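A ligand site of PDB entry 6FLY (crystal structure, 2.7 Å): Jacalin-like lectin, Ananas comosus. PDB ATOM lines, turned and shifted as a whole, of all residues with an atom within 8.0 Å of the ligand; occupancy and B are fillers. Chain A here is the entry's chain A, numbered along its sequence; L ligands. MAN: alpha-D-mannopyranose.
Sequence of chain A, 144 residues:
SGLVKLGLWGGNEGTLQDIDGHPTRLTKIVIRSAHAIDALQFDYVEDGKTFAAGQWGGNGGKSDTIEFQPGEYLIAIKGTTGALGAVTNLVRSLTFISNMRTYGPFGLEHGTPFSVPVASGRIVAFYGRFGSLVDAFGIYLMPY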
ATOM      1  N   GLY A  11      12.133   6.507  32.601  1.00  0.00           N
ATOM      2  CA  GLY A  11      13.504   6.038  32.581  1.00  0.00           C
ATOM      3  C   GLY A  11      14.496   7.111  32.165  1.00  0.00           C
ATOM      4  O   GLY A  11      14.170   8.299  32.015  1.00  0.00           O
ATOM      5  N   ASN A  12      15.730   6.670  31.952  1.00  0.00           N
ATOM      6  CA  ASN A  12      16.882   7.538  31.758  1.00  0.00           C
ATOM      7  C   ASN A  12      17.369   7.539  30.316  1.00  0.00           C
ATOM      8  O   ASN A  12      18.384   8.181  30.034  1.00  0.00           O
ATOM      9  CB  ASN A  12      18.016   7.135  32.695  1.00  0.00           C
ATOM     10  CG  ASN A  12      17.605   7.174  34.149  1.00  0.00           C
ATOM     11  OD1 ASN A  12      16.847   8.054  34.565  1.00  0.00           O
ATOM     12  ND2 ASN A  12      18.088   6.214  34.939  1.00  0.00           N
ATOM     13  N   GLU A  13      16.684   6.855  29.412  1.00  0.00           N
ATOM     14  CA  GLU A  13      17.174   6.739  28.049  1.00  0.00           C
ATOM     15  C   GLU A  13      16.489   7.802  27.183  1.00  0.00           C
ATOM     16  O   GLU A  13      15.926   8.771  27.692  1.00  0.00           O
ATOM     17  CB  GLU A  13      16.889   5.318  27.545  1.00  0.00           C
ATOM     18  CG  GLU A  13      17.580   4.220  28.333  1.00  0.00           C
ATOM     19  CD  GLU A  13      19.078   4.369  28.369  1.00  0.00           C
ATOM     20  OE1 GLU A  13      19.658   4.763  27.328  1.00  0.00           O
ATOM     21  OE2 GLU A  13      19.686   4.102  29.425  1.00  0.00           O
ATOM     22  N   GLY A  14      16.535   7.625  25.866  1.00  0.00           N
ATOM     23  CA  GLY A  14      16.126   8.692  24.989  1.00  0.00           C
ATOM     24  C   GLY A  14      16.951   9.958  25.206  1.00  0.00           C
ATOM     25  O   GLY A  14      18.065   9.942  25.751  1.00  0.00           O
ATOM     26  N   THR A  15      16.372  11.067  24.756  1.00  0.00           N
ATOM     27  CA  THR A  15      16.994  12.382  24.806  1.00  0.00           C
ATOM     28  C   THR A  15      16.014  13.352  25.431  1.00  0.00           C
ATOM     29  O   THR A  15      14.814  13.332  25.128  1.00  0.00           O
ATOM     30  CB  THR A  15      17.407  12.852  23.403  1.00  0.00           C
ATOM     31  OG1 THR A  15      18.371  11.945  22.855  1.00  0.00           O
ATOM     32  CG2 THR A  15      17.993  14.268  23.445  1.00  0.00           C
ATOM     33  N   ILE A  37       3.259   4.839  25.120  1.00  0.00           N
ATOM     34  CA  ILE A  37       3.099   6.178  24.575  1.00  0.00           C
ATOM     35  C   ILE A  37       4.265   6.420  23.613  1.00  0.00           C
ATOM     36  O   ILE A  37       5.428   6.428  24.025  1.00  0.00           O
ATOM     37  CB  ILE A  37       3.074   7.243  25.682  1.00  0.00           C
ATOM     38  CG1 ILE A  37       2.004   6.930  26.731  1.00  0.00           C
ATOM     39  CG2 ILE A  37       2.796   8.617  25.098  1.00  0.00           C
ATOM     40  CD1 ILE A  37       0.631   6.626  26.177  1.00  0.00           C
ATOM     41  N   ASP A  38       3.939   6.640  22.340  1.00  0.00           N
ATOM     42  CA  ASP A  38       4.933   6.815  21.279  1.00  0.00           C
ATOM     43  C   ASP A  38       5.454   8.245  21.138  1.00  0.00           C
ATOM     44  O   ASP A  38       6.659   8.436  20.930  1.00  0.00           O
ATOM     45  CB  ASP A  38       4.347   6.364  19.943  1.00  0.00           C
ATOM     46  CG  ASP A  38       4.207   4.860  19.836  1.00  0.00           C
ATOM     47  OD1 ASP A  38       3.189   4.316  20.306  1.00  0.00           O
ATOM     48  OD2 ASP A  38       5.132   4.223  19.277  1.00  0.00           O
ATOM     49  N   GLY A  57       9.261  12.324  20.155  1.00  0.00           N
ATOM     50  CA  GLY A  57       9.044  10.891  20.051  1.00  0.00           C
ATOM     51  C   GLY A  57       8.952  10.435  18.599  1.00  0.00           C
ATOM     52  O   GLY A  57       9.179  11.202  17.658  1.00  0.00           O
ATOM     53  N   GLY A  58       8.616   9.156  18.435  1.00  0.00           N
ATOM     54  CA  GLY A  58       8.643   8.509  17.139  1.00  0.00           C
ATOM     55  C   GLY A  58       7.302   8.582  16.431  1.00  0.00           C
ATOM     56  O   GLY A  58       6.368   9.260  16.859  1.00  0.00           O
ATOM     57  N   LEU A  84       9.077  -2.283  28.412  1.00  0.00           N
ATOM     58  CA  LEU A  84       8.506  -2.758  27.162  1.00  0.00           C
ATOM     59  C   LEU A  84       9.671  -3.233  26.322  1.00  0.00           C
ATOM     60  O   LEU A  84      10.587  -2.461  26.036  1.00  0.00           O
ATOM     61  CB  LEU A  84       7.773  -1.637  26.416  1.00  0.00           C
ATOM     62  CG  LEU A  84       7.035  -2.027  25.126  1.00  0.00           C
ATOM     63  CD1 LEU A  84       5.796  -2.871  25.400  1.00  0.00           C
ATOM     64  CD2 LEU A  84       6.707  -0.790  24.288  1.00  0.00           C
ATOM     65  N   ALA A  86      12.942  -4.221  25.000  1.00  0.00           N
ATOM     66  CA  ALA A  86      14.300  -3.938  25.399  1.00  0.00           C
ATOM     67  C   ALA A  86      14.427  -2.652  26.209  1.00  0.00           C
ATOM     68  O   ALA A  86      15.541  -2.325  26.645  1.00  0.00           O
ATOM     69  CB  ALA A  86      15.196  -3.864  24.169  1.00  0.00           C
ATOM     70  N   VAL A  87      13.343  -1.899  26.408  1.00  0.00           N
ATOM     71  CA  VAL A  87      13.433  -0.633  27.118  1.00  0.00           C
ATOM     72  C   VAL A  87      13.118  -0.943  28.571  1.00  0.00           C
ATOM     73  O   VAL A  87      12.038  -1.464  28.893  1.00  0.00           O
ATOM     74  CB  VAL A  87      12.461   0.416  26.546  1.00  0.00           C
ATOM     75  CG1 VAL A  87      12.589   1.732  27.310  1.00  0.00           C
ATOM     76  CG2 VAL A  87      12.730   0.657  25.070  1.00  0.00           C
ATOM     77  N   THR A  88      14.058  -0.612  29.458  1.00  0.00           N
ATOM     78  CA  THR A  88      13.906  -0.956  30.867  1.00  0.00           C
ATOM     79  C   THR A  88      12.743  -0.228  31.515  1.00  0.00           C
ATOM     80  O   THR A  88      12.052  -0.794  32.372  1.00  0.00           O
ATOM     81  CB  THR A  88      15.205  -0.632  31.607  1.00  0.00           C
ATOM     82  OG1 THR A  88      16.267  -1.447  31.106  1.00  0.00           O
ATOM     83  CG2 THR A  88      15.036  -0.869  33.106  1.00  0.00           C
ATOM     84  N   ASN A  89      12.524   1.033  31.174  1.00  0.00           N
ATOM     85  CA  ASN A  89      11.519   1.830  31.860  1.00  0.00           C
ATOM     86  C   ASN A  89      11.115   3.004  30.975  1.00  0.00           C
ATOM     87  O   ASN A  89      11.944   3.881  30.698  1.00  0.00           O
ATOM     88  CB  ASN A  89      12.082   2.319  33.197  1.00  0.00           C
ATOM     89  CG  ASN A  89      11.046   2.979  34.078  1.00  0.00           C
ATOM     90  OD1 ASN A  89       9.836   2.763  33.921  1.00  0.00           O
ATOM     91  ND2 ASN A  89      11.503   3.765  35.033  1.00  0.00           N
ATOM     92  N   LEU A  90       9.865   3.018  30.542  1.00  0.00           N
ATOM     93  CA  LEU A  90       9.314   4.090  29.714  1.00  0.00           C
ATOM     94  C   LEU A  90       7.874   4.328  30.154  1.00  0.00           C
ATOM     95  O   LEU A  90       7.364   3.681  31.076  1.00  0.00           O
ATOM     96  CB  LEU A  90       9.442   3.783  28.225  1.00  0.00           C
ATOM     97  CG  LEU A  90       8.947   2.455  27.639  1.00  0.00           C
ATOM     98  CD1 LEU A  90       7.476   2.204  27.917  1.00  0.00           C
ATOM     99  CD2 LEU A  90       9.180   2.438  26.138  1.00  0.00           C
ATOM    100  N   ARG A 129      11.679  12.828  28.194  1.00  0.00           N
ATOM    101  CA  ARG A 129      12.759  12.191  27.455  1.00  0.00           C
ATOM    102  C   ARG A 129      12.136  11.288  26.395  1.00  0.00           C
ATOM    103  O   ARG A 129      11.170  10.566  26.681  1.00  0.00           O
ATOM    104  CB  ARG A 129      13.694  11.377  28.371  1.00  0.00           C
ATOM    105  CG  ARG A 129      14.306  12.172  29.513  1.00  0.00           C
ATOM    106  CD  ARG A 129      15.304  11.341  30.296  1.00  0.00           C
ATOM    107  NE  ARG A 129      16.452  10.935  29.484  1.00  0.00           N
ATOM    108  CZ  ARG A 129      17.578  11.630  29.350  1.00  0.00           C
ATOM    109  NH1 ARG A 129      17.749  12.781  30.002  1.00  0.00           N
ATOM    110  NH2 ARG A 129      18.557  11.175  28.581  1.00  0.00           N
ATOM    111  N   PHE A 130      12.724  11.310  25.206  1.00  0.00           N
ATOM    112  CA  PHE A 130      12.100  10.743  24.015  1.00  0.00           C
ATOM    113  C   PHE A 130      13.144  10.107  23.109  1.00  0.00           C
ATOM    114  O   PHE A 130      14.225  10.666  22.907  1.00  0.00           O
ATOM    115  CB  PHE A 130      11.366  11.827  23.207  1.00  0.00           C
ATOM    116  CG  PHE A 130      10.377  12.615  24.006  1.00  0.00           C
ATOM    117  CD1 PHE A 130      10.782  13.726  24.732  1.00  0.00           C
ATOM    118  CD2 PHE A 130       9.039  12.259  24.034  1.00  0.00           C
ATOM    119  CE1 PHE A 130       9.865  14.456  25.470  1.00  0.00           C
ATOM    120  CE2 PHE A 130       8.122  12.981  24.765  1.00  0.00           C
ATOM    121  CZ  PHE A 130       8.538  14.089  25.482  1.00  0.00           C
ATOM    122  N   GLY A 131      12.788   8.961  22.557  1.00  0.00           N
ATOM    123  CA  GLY A 131      13.548   8.355  21.480  1.00  0.00           C
ATOM    124  C   GLY A 131      12.555   7.939  20.414  1.00  0.00           C
ATOM    125  O   GLY A 131      11.848   8.794  19.876  1.00  0.00           O
ATOM    126  N   SER A 132      12.476   6.656  20.085  1.00  0.00           N
ATOM    127  CA  SER A 132      11.367   6.217  19.245  1.00  0.00           C
ATOM    128  C   SER A 132      10.061   6.181  20.031  1.00  0.00           C
ATOM    129  O   SER A 132       8.987   6.143  19.431  1.00  0.00           O
ATOM    130  CB  SER A 132      11.659   4.842  18.642  1.00  0.00           C
ATOM    131  OG  SER A 132      11.949   3.900  19.663  1.00  0.00           O
ATOM    132  N   LEU A 133      10.144   6.208  21.363  1.00  0.00           N
ATOM    133  CA  LEU A 133       8.983   6.251  22.246  1.00  0.00           C
ATOM    134  C   LEU A 133       9.189   7.356  23.285  1.00  0.00           C
ATOM    135  O   LEU A 133      10.186   8.090  23.267  1.00  0.00           O
ATOM    136  CB  LEU A 133       8.779   4.893  22.920  1.00  0.00           C
ATOM    137  CG  LEU A 133       8.650   3.710  21.959  1.00  0.00           C
ATOM    138  CD1 LEU A 133       8.686   2.397  22.722  1.00  0.00           C
ATOM    139  CD2 LEU A 133       7.346   3.818  21.176  1.00  0.00           C
ATOM    140  N   VAL A 134       8.222   7.480  24.197  1.00  0.00           N
ATOM    141  CA  VAL A 134       8.318   8.414  25.312  1.00  0.00           C
ATOM    142  C   VAL A 134       9.004   7.696  26.471  1.00  0.00           C
ATOM    143  O   VAL A 134       8.369   6.901  27.182  1.00  0.00           O
ATOM    144  CB  VAL A 134       6.950   8.960  25.716  1.00  0.00           C
ATOM    145  CG1 VAL A 134       7.081   9.943  26.871  1.00  0.00           C
ATOM    146  CG2 VAL A 134       6.264   9.625  24.524  1.00  0.00           C
ATOM    147  N   ASP A 135      10.291   7.961  26.661  1.00  0.00           N
ATOM    148  CA  ASP A 135      11.024   7.356  27.768  1.00  0.00           C
ATOM    149  C   ASP A 135      10.589   7.939  29.117  1.00  0.00           C
ATOM    150  O   ASP A 135      10.498   7.211  30.109  1.00  0.00           O
ATOM    151  CB  ASP A 135      12.522   7.512  27.565  1.00  0.00           C
ATOM    152  CG  ASP A 135      13.048   6.662  26.419  1.00  0.00           C
ATOM    153  OD1 ASP A 135      13.016   7.139  25.266  1.00  0.00           O
ATOM    154  OD2 ASP A 135      13.458   5.518  26.680  1.00  0.00           O
ATOM    155  N   ALA A 136      10.311   9.241  29.174  1.00  0.00           N
ATOM    156  CA  ALA A 136       9.985   9.868  30.448  1.00  0.00           C
ATOM    157  C   ALA A 136       9.136  11.109  30.200  1.00  0.00           C
ATOM    158  O   ALA A 136       9.140  11.681  29.113  1.00  0.00           O
ATOM    159  CB  ALA A 136      11.261  10.222  31.226  1.00  0.00           C
HETATM  160  C1  MAN L   1      15.375   4.783  20.807  1.00  0.00           C
HETATM  161  C2  MAN L   1      16.621   5.238  21.606  1.00  0.00           C
HETATM  162  C3  MAN L   1      16.580   4.723  23.063  1.00  0.00           C
HETATM  163  C4  MAN L   1      15.174   4.817  23.687  1.00  0.00           C
HETATM  164  C5  MAN L   1      14.136   4.222  22.729  1.00  0.00           C
HETATM  165  C6  MAN L   1      12.704   4.291  23.243  1.00  0.00           C
HETATM  166  O1  MAN L   1      15.612   3.443  20.451  1.00  0.00           O
HETATM  167  O2  MAN L   1      16.696   6.660  21.687  1.00  0.00           O
HETATM  168  O3  MAN L   1      17.524   5.413  23.881  1.00  0.00           O
HETATM  169  O4  MAN L   1      15.151   4.105  24.917  1.00  0.00           O
HETATM  170  O5  MAN L   1      14.180   4.941  21.509  1.00  0.00           O
HETATM  171  O6  MAN L   1      12.211   5.609  23.022  1.00  0.00           O
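CB of Glu 13 touches O4 of the ligand, 3.4 Å away. Hydrophobic or aromatic side chains that line the ligand: Leu 133. Within 4 Å of the ligand: Glu 13, Gly 14, Gly 131, Ser 132, Leu 133 and Asp 135. The nearest printed residue that does not touch the ligand is Val 87 (4.1 Å).
O of Ser 132 sits at hydrogen-bond distance from N of Gly 58 (3.2 Å). The backbone NH (N) of Gly 131 lies within hydrogen-bond range of the side-chain carboxylate (OD1) of Asp 135, 3.3 Å away. The backbone NH (N) of Asp 135 sits at hydrogen-bond distance from the backbone carbonyl oxygen (O) of Arg 129 (2.7 Å). O of Asp 135 is in hydrogen-bond range of N of Gly 11 (3.1 Å). The backbone carbonyl oxygen (O) of Gly 14 is in hydrogen-bond range of the guanidinium group (NH2) of Arg 129 (3.1 Å). The guanidinium group (NE) of Arg 129 is in hydrogen-bond range of the backbone carbonyl oxygen (O) of Glu 13 (2.9 Å).
The backbone NH of Leu 133 lies within hydrogen-bond range of an oxygen (O6) of the ligand (2.7 Å). O of Leu 133 is in hydrogen-bond range of O6 of the ligand (3.2 Å). An oxygen (O5) of the ligand lies within hydrogen-bond range of the backbone NH (N) of Ser 132, 2.8 Å away. The side-chain hydroxyl (OG) of Ser 132 sits at hydrogen-bond distance from an oxygen (O5) of the ligand. OD2 of Asp 135 is in hydrogen-bond range of O4 of the ligand (2.8 Å). O3 of the ligand lies within hydrogen-bond range of N of Gly 14 (3.1 Å). The backbone NH of Gly 131 sits close to an oxygen (O6) of the ligand, at 3.4 Å.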
